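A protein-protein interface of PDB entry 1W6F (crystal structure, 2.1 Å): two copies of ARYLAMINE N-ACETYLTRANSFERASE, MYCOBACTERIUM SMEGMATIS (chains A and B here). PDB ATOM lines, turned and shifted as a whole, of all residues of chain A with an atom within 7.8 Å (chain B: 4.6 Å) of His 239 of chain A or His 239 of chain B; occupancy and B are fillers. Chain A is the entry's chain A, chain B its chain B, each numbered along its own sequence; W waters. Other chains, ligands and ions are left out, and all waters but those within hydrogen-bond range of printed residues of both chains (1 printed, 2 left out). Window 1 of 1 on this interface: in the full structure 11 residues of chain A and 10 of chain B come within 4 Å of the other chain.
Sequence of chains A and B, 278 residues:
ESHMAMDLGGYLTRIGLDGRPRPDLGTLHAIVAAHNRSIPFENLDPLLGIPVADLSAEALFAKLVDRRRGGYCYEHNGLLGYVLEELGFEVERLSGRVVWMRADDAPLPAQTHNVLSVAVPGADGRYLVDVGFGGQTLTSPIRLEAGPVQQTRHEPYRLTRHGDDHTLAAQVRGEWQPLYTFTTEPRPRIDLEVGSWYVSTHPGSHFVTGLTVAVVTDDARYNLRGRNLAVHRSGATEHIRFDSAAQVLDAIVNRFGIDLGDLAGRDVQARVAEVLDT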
ATOM      1  N   ASN A 223       7.002   7.436  -4.741  1.00  0.00           N
ATOM      2  CA  ASN A 223       7.145   8.591  -3.881  1.00  0.00           C
ATOM      3  C   ASN A 223       7.209   9.853  -4.678  1.00  0.00           C
ATOM      4  O   ASN A 223       8.163  10.042  -5.396  1.00  0.00           O
ATOM      5  CB  ASN A 223       8.382   8.541  -2.984  1.00  0.00           C
ATOM      6  CG  ASN A 223       8.381   9.720  -1.927  1.00  0.00           C
ATOM      7  OD1 ASN A 223       7.363  10.040  -1.296  1.00  0.00           O
ATOM      8  ND2 ASN A 223       9.487  10.379  -1.812  1.00  0.00           N
ATOM      9  N   ARG A 227       7.197  18.080  -8.194  1.00  0.00           N
ATOM     10  CA  ARG A 227       7.156  17.563  -9.564  1.00  0.00           C
ATOM     11  C   ARG A 227       7.893  16.231  -9.751  1.00  0.00           C
ATOM     12  O   ARG A 227       7.840  15.651 -10.809  1.00  0.00           O
ATOM     13  CB  ARG A 227       7.747  18.586 -10.576  1.00  0.00           C
ATOM     14  CG  ARG A 227       9.203  18.825 -10.415  1.00  0.00           C
ATOM     15  CD  ARG A 227       9.843  19.622 -11.571  1.00  0.00           C
ATOM     16  NE  ARG A 227       9.788  21.061 -11.328  1.00  0.00           N
ATOM     17  CZ  ARG A 227       9.171  21.944 -12.094  1.00  0.00           C
ATOM     18  NH1 ARG A 227       8.534  21.567 -13.175  1.00  0.00           N
ATOM     19  NH2 ARG A 227       9.225  23.243 -11.800  1.00  0.00           N
ATOM     20  N   ASN A 228       8.669  15.819  -8.776  1.00  0.00           N
ATOM     21  CA  ASN A 228       9.509  14.622  -8.912  1.00  0.00           C
ATOM     22  C   ASN A 228       8.856  13.363  -8.354  1.00  0.00           C
ATOM     23  O   ASN A 228       8.545  13.316  -7.151  1.00  0.00           O
ATOM     24  CB  ASN A 228      10.795  14.904  -8.231  1.00  0.00           C
ATOM     25  CG  ASN A 228      11.497  16.147  -8.817  1.00  0.00           C
ATOM     26  OD1 ASN A 228      11.799  16.153  -9.996  1.00  0.00           O
ATOM     27  ND2 ASN A 228      11.775  17.135  -8.004  1.00  0.00           N
ATOM     28  N   LEU A 229       8.583  12.389  -9.217  1.00  0.00           N
ATOM     29  CA  LEU A 229       8.113  11.095  -8.830  1.00  0.00           C
ATOM     30  C   LEU A 229       9.259  10.117  -8.876  1.00  0.00           C
ATOM     31  O   LEU A 229       9.803   9.853  -9.928  1.00  0.00           O
ATOM     32  CB  LEU A 229       7.008  10.621  -9.793  1.00  0.00           C
ATOM     33  CG  LEU A 229       6.445   9.234  -9.607  1.00  0.00           C
ATOM     34  CD1 LEU A 229       6.022   8.989  -8.174  1.00  0.00           C
ATOM     35  CD2 LEU A 229       5.266   9.000 -10.597  1.00  0.00           C
ATOM     36  N   ALA A 230       9.630   9.555  -7.746  1.00  0.00           N
ATOM     37  CA  ALA A 230      10.592   8.447  -7.683  1.00  0.00           C
ATOM     38  C   ALA A 230       9.882   7.089  -7.486  1.00  0.00           C
ATOM     39  O   ALA A 230       8.931   7.002  -6.702  1.00  0.00           O
ATOM     40  CB  ALA A 230      11.635   8.744  -6.581  1.00  0.00           C
ATOM     41  N   VAL A 231      10.269   6.071  -8.252  1.00  0.00           N
ATOM     42  CA  VAL A 231       9.724   4.701  -8.162  1.00  0.00           C
ATOM     43  C   VAL A 231      10.934   3.785  -7.909  1.00  0.00           C
ATOM     44  O   VAL A 231      11.903   3.780  -8.677  1.00  0.00           O
ATOM     45  CB  VAL A 231       8.961   4.320  -9.462  1.00  0.00           C
ATOM     46  CG1 VAL A 231       8.061   3.087  -9.298  1.00  0.00           C
ATOM     47  CG2 VAL A 231       8.113   5.507  -9.944  1.00  0.00           C
ATOM     48  N   HIS A 232      10.958   3.091  -6.796  1.00  0.00           N
ATOM     49  CA  HIS A 232      12.040   2.155  -6.508  1.00  0.00           C
ATOM     50  C   HIS A 232      11.458   0.778  -6.772  1.00  0.00           C
ATOM     51  O   HIS A 232      10.462   0.407  -6.138  1.00  0.00           O
ATOM     52  CB  HIS A 232      12.453   2.257  -5.036  1.00  0.00           C
ATOM     53  CG  HIS A 232      13.218   3.488  -4.679  1.00  0.00           C
ATOM     54  ND1 HIS A 232      14.096   3.523  -3.604  1.00  0.00           N
ATOM     55  CD2 HIS A 232      13.220   4.736  -5.209  1.00  0.00           C
ATOM     56  CE1 HIS A 232      14.596   4.743  -3.496  1.00  0.00           C
ATOM     57  NE2 HIS A 232      14.097   5.490  -4.474  1.00  0.00           N
ATOM     58  N   ALA A 236      16.001  -1.462 -10.439  1.00  0.00           N
ATOM     59  CA  ALA A 236      15.974  -0.171 -11.056  1.00  0.00           C
ATOM     60  C   ALA A 236      15.263   0.890 -10.196  1.00  0.00           C
ATOM     61  O   ALA A 236      14.290   0.607  -9.483  1.00  0.00           O
ATOM     62  CB  ALA A 236      15.275  -0.287 -12.410  1.00  0.00           C
ATOM     63  N   THR A 237      15.706   2.123 -10.333  1.00  0.00           N
ATOM     64  CA  THR A 237      14.946   3.283  -9.917  1.00  0.00           C
ATOM     65  C   THR A 237      14.495   4.128 -11.082  1.00  0.00           C
ATOM     66  O   THR A 237      15.270   4.363 -12.020  1.00  0.00           O
ATOM     67  CB  THR A 237      15.821   4.126  -8.998  1.00  0.00           C
ATOM     68  OG1 THR A 237      16.024   3.396  -7.784  1.00  0.00           O
ATOM     69  CG2 THR A 237      15.076   5.367  -8.511  1.00  0.00           C
ATOM     70  N   GLU A 238      13.256   4.608 -11.039  1.00  0.00           N
ATOM     71  CA  GLU A 238      12.775   5.580 -12.005  1.00  0.00           C
ATOM     72  C   GLU A 238      12.557   6.949 -11.358  1.00  0.00           C
ATOM     73  O   GLU A 238      12.162   7.067 -10.161  1.00  0.00           O
ATOM     74  CB  GLU A 238      11.496   5.167 -12.679  1.00  0.00           C
ATOM     75  CG  GLU A 238      11.299   3.685 -12.899  1.00  0.00           C
ATOM     76  CD  GLU A 238       9.889   3.382 -13.399  1.00  0.00           C
ATOM     77  OE1 GLU A 238       9.108   4.350 -13.693  1.00  0.00           O
ATOM     78  OE2 GLU A 238       9.555   2.172 -13.486  1.00  0.00           O
ATOM     79  N   HIS A 239      12.889   7.981 -12.109  1.00  0.00           N
ATOM     80  CA  HIS A 239      12.690   9.364 -11.696  1.00  0.00           C
ATOM     81  C   HIS A 239      11.866   9.980 -12.806  1.00  0.00           C
ATOM     82  O   HIS A 239      12.321  10.052 -13.969  1.00  0.00           O
ATOM     83  CB  HIS A 239      13.989  10.107 -11.440  1.00  0.00           C
ATOM     84  CG  HIS A 239      14.775   9.574 -10.267  1.00  0.00           C
ATOM     85  ND1 HIS A 239      14.275   9.526  -8.976  1.00  0.00           N
ATOM     86  CD2 HIS A 239      16.036   9.069 -10.190  1.00  0.00           C
ATOM     87  CE1 HIS A 239      15.185   9.004  -8.169  1.00  0.00           C
ATOM     88  NE2 HIS A 239      16.263   8.721  -8.880  1.00  0.00           N
ATOM     89  N   ILE A 240      10.622  10.356 -12.508  1.00  0.00           N
ATOM     90  CA  ILE A 240       9.799  11.046 -13.502  1.00  0.00           C
ATOM     91  C   ILE A 240       9.721  12.497 -13.034  1.00  0.00           C
ATOM     92  O   ILE A 240       9.361  12.772 -11.860  1.00  0.00           O
ATOM     93  CB  ILE A 240       8.430  10.416 -13.643  1.00  0.00           C
ATOM     94  CG1 ILE A 240       8.549   8.987 -14.160  1.00  0.00           C
ATOM     95  CG2 ILE A 240       7.491  11.235 -14.555  1.00  0.00           C
ATOM     96  CD1 ILE A 240       7.310   8.219 -14.138  1.00  0.00           C
ATOM     97  N   ARG A 241      10.054  13.430 -13.938  1.00  0.00           N
ATOM     98  CA  ARG A 241       9.977  14.860 -13.645  1.00  0.00           C
ATOM     99  C   ARG A 241       8.841  15.444 -14.454  1.00  0.00           C
ATOM    100  O   ARG A 241       8.863  15.443 -15.701  1.00  0.00           O
ATOM    101  CB  ARG A 241      11.289  15.550 -13.938  1.00  0.00           C
ATOM    102  CG  ARG A 241      11.375  16.993 -13.484  1.00  0.00           C
ATOM    103  CD  ARG A 241      12.675  17.665 -14.032  1.00  0.00           C
ATOM    104  NE  ARG A 241      12.764  19.036 -13.632  1.00  0.00           N
ATOM    105  CZ  ARG A 241      12.131  20.026 -14.220  1.00  0.00           C
ATOM    106  NH1 ARG A 241      11.364  19.825 -15.287  1.00  0.00           N
ATOM    107  NH2 ARG A 241      12.300  21.230 -13.740  1.00  0.00           N
ATOM    108  N   PHE A 242       7.800  15.833 -13.766  1.00  0.00           N
ATOM    109  CA  PHE A 242       6.662  16.468 -14.444  1.00  0.00           C
ATOM    110  C   PHE A 242       6.960  17.911 -14.836  1.00  0.00           C
ATOM    111  O   PHE A 242       7.678  18.622 -14.154  1.00  0.00           O
ATOM    112  CB  PHE A 242       5.412  16.371 -13.609  1.00  0.00           C
ATOM    113  CG  PHE A 242       4.961  14.975 -13.397  1.00  0.00           C
ATOM    114  CD1 PHE A 242       5.012  14.401 -12.132  1.00  0.00           C
ATOM    115  CD2 PHE A 242       4.507  14.187 -14.473  1.00  0.00           C
ATOM    116  CE1 PHE A 242       4.576  13.102 -11.955  1.00  0.00           C
ATOM    117  CE2 PHE A 242       4.072  12.901 -14.274  1.00  0.00           C
ATOM    118  CZ  PHE A 242       4.126  12.361 -13.002  1.00  0.00           C
ATOM    119  N   LEU B 229      18.501   5.086 -18.737  1.00  0.00           N
ATOM    120  CA  LEU B 229      17.507   5.141 -19.788  1.00  0.00           C
ATOM    121  C   LEU B 229      16.720   6.420 -19.640  1.00  0.00           C
ATOM    122  O   LEU B 229      16.144   6.701 -18.561  1.00  0.00           O
ATOM    123  CB  LEU B 229      16.587   3.950 -19.717  1.00  0.00           C
ATOM    124  CG  LEU B 229      15.449   3.931 -20.716  1.00  0.00           C
ATOM    125  CD1 LEU B 229      15.984   3.851 -22.103  1.00  0.00           C
ATOM    126  CD2 LEU B 229      14.527   2.735 -20.504  1.00  0.00           C
ATOM    127  N   ALA B 230      16.716   7.245 -20.679  1.00  0.00           N
ATOM    128  CA  ALA B 230      15.884   8.445 -20.698  1.00  0.00           C
ATOM    129  C   ALA B 230      14.691   8.220 -21.596  1.00  0.00           C
ATOM    130  O   ALA B 230      14.778   7.525 -22.602  1.00  0.00           O
ATOM    131  CB  ALA B 230      16.695   9.687 -21.114  1.00  0.00           C
ATOM    132  N   THR B 237       9.756  14.240 -18.405  1.00  0.00           N
ATOM    133  CA  THR B 237      10.942  13.462 -18.694  1.00  0.00           C
ATOM    134  C   THR B 237      11.137  12.380 -17.641  1.00  0.00           C
ATOM    135  O   THR B 237      11.037  12.618 -16.467  1.00  0.00           O
ATOM    136  CB  THR B 237      12.218  14.351 -18.861  1.00  0.00           C
ATOM    137  OG1 THR B 237      12.322  15.345 -17.816  1.00  0.00           O
ATOM    138  CG2 THR B 237      12.104  15.177 -20.077  1.00  0.00           C
ATOM    139  N   GLU B 238      11.467  11.196 -18.111  1.00  0.00           N
ATOM    140  CA  GLU B 238      11.540   9.997 -17.329  1.00  0.00           C
ATOM    141  C   GLU B 238      12.995   9.454 -17.376  1.00  0.00           C
ATOM    142  O   GLU B 238      13.588   9.359 -18.454  1.00  0.00           O
ATOM    143  CB  GLU B 238      10.514   9.072 -17.933  1.00  0.00           C
ATOM    144  CG  GLU B 238      10.130   7.875 -17.111  1.00  0.00           C
ATOM    145  CD  GLU B 238       9.054   7.013 -17.780  1.00  0.00           C
ATOM    146  OE1 GLU B 238       9.305   5.779 -17.913  1.00  0.00           O
ATOM    147  OE2 GLU B 238       7.970   7.565 -18.156  1.00  0.00           O
ATOM    148  N   HIS B 239      13.602   9.193 -16.226  1.00  0.00           N
ATOM    149  CA  HIS B 239      14.984   8.698 -16.116  1.00  0.00           C
ATOM    150  C   HIS B 239      15.022   7.408 -15.314  1.00  0.00           C
ATOM    151  O   HIS B 239      14.776   7.401 -14.072  1.00  0.00           O
ATOM    152  CB  HIS B 239      15.979   9.742 -15.533  1.00  0.00           C
ATOM    153  CG  HIS B 239      16.037  11.038 -16.317  1.00  0.00           C
ATOM    154  ND1 HIS B 239      16.138  11.076 -17.700  1.00  0.00           N
ATOM    155  CD2 HIS B 239      16.035  12.333 -15.914  1.00  0.00           C
ATOM    156  CE1 HIS B 239      16.143  12.331 -18.111  1.00  0.00           C
ATOM    157  NE2 HIS B 239      16.083  13.114 -17.047  1.00  0.00           N
ATOM    158  N   ILE B 240      15.263   6.300 -16.017  1.00  0.00           N
ATOM    159  CA  ILE B 240      15.429   5.010 -15.365  1.00  0.00           C
ATOM    160  C   ILE B 240      16.899   4.688 -15.173  1.00  0.00           C
ATOM    161  O   ILE B 240      17.677   4.726 -16.165  1.00  0.00           O
ATOM    162  CB  ILE B 240      14.694   3.952 -16.156  1.00  0.00           C
ATOM    163  CG1 ILE B 240      13.231   4.362 -16.282  1.00  0.00           C
ATOM    164  CG2 ILE B 240      14.873   2.582 -15.484  1.00  0.00           C
ATOM    165  CD1 ILE B 240      12.397   3.491 -17.157  1.00  0.00           C
ATOM    166  N   ARG B 241      17.332   4.534 -13.909  1.00  0.00           N
ATOM    167  CA  ARG B 241      18.668   4.052 -13.616  1.00  0.00           C
ATOM    168  C   ARG B 241      18.675   2.563 -13.249  1.00  0.00           C
ATOM    169  O   ARG B 241      18.143   2.160 -12.198  1.00  0.00           O
ATOM    170  CB  ARG B 241      19.293   4.877 -12.500  1.00  0.00           C
ATOM    171  CG  ARG B 241      20.724   4.534 -12.127  1.00  0.00           C
ATOM    172  CD  ARG B 241      21.165   5.194 -10.794  1.00  0.00           C
ATOM    173  NE  ARG B 241      22.579   4.950 -10.547  1.00  0.00           N
ATOM    174  CZ  ARG B 241      23.090   3.837 -10.035  1.00  0.00           C
ATOM    175  NH1 ARG B 241      22.321   2.804  -9.672  1.00  0.00           N
ATOM    176  NH2 ARG B 241      24.404   3.744  -9.896  1.00  0.00           N
HETATM  177  O   HOH W   1      10.293  17.482 -16.754  1.00  0.00           O
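The backbone carbonyl oxygen of Thr 237 of chain A sits at hydrogen-bond distance from the backbone NH of Arg 241 of chain B, 2.8 Å away.
The backbone NH (N) of His 239 of chain B lies within hydrogen-bond range of the backbone carbonyl oxygen (O) of His 239 of chain A, at 2.7 Å.
N of Arg 241 of chain A sits at hydrogen-bond distance from O of Thr 237 of chain B (2.8 Å).
O of Leu 229 of chain A lies within hydrogen-bond range of N of Ile 240 of chain A, at 2.8 Å.
The backbone carbonyl oxygen (O) of Val 231 of chain A lies within hydrogen-bond range of the backbone NH (N) of Glu 238 of chain A, at 2.8 Å.
The backbone carbonyl oxygen (O) of Leu 229 of chain B lies within hydrogen-bond range of the backbone NH (N) of Ile 240 of chain B, at 2.7 Å.
Among the printed residues, pairs that only touch across the chains: Ala 236 of chain A with Arg 241 of chain B, Glu 238 of chain A with His 239 of chain B, Thr 237 of chain A with Ile 240 of chain B, His 239 of chain A with Glu 238 of chain B, Ile 240 of chain A with Glu 238 of chain B, Ile 240 of chain A with Thr 237 of chain B, Thr 237 of chain A with His 239 of chain B, His 239 of chain A with Thr 237 of chain B and Glu 238 of chain A with Ile 240 of chain B.
His 239 of chain A touches just these residues of chain B: Thr 237, Glu 238 and His 239.
Of the printed residues of chain B, Ile 240 of chain A touches Thr 237 and Glu 238.
Of the printed residues of chain B, Arg 241 of chain A touches Thr 237 (2.8 Å).
Of the printed residues of chain A, Thr 237 of chain B touches His 239 (3.8 Å), Ile 240 (3.6 Å) and Arg 241 (2.8 Å).
His 239 of chain B touches just these residues of chain A: Thr 237 (3.7 Å), Glu 238 (3.4 Å) and His 239 (2.7 Å).
The nearest printed residue of chain B that does not touch His 239 of chain A is Ile 240 of chain B (4.9 Å).
The nearest residue of chain A that does not touch His 239 of chain B is Ile 240 of chain A (4.9 Å).
Of the 7 printed residues of chain B, 5 touch a printed residue of chain A.
Hydrophobic or aromatic side chains of chain B within 4 Å of the printed part of chain A: His 239 and Ile 240.
Among the printed residues, no Asp or Glu carboxylate lies within 4 Å of a Lys or Arg side-chain nitrogen of the other chain.
Thr 237 of chain A touches His 239 of chain B, and with the chains exchanged His 239 of chain A touches Thr 237 of chain B.
Thr 237 of chain A touches Arg 241 of chain B, and with the chains exchanged Arg 241 of chain A touches Thr 237 of chain B.
Glu 238 of chain A touches His 239 of chain B, and with the chains exchanged His 239 of chain A touches Glu 238 of chain B.
Glu 238 of chain A touches Ile 240 of chain B, and with the chains exchanged Ile 240 of chain A touches Glu 238 of chain B.
Positions printed for both chains: 229, 230, 237, 238, 239, 240 and 241.
Of the 12 pairs that touch across the chains among the printed residues, 11 have their exchanged pair printed and touching as well.
Water W1 bridges O of Arg 241 of chain A and OG1 of Thr 237 of chain B.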
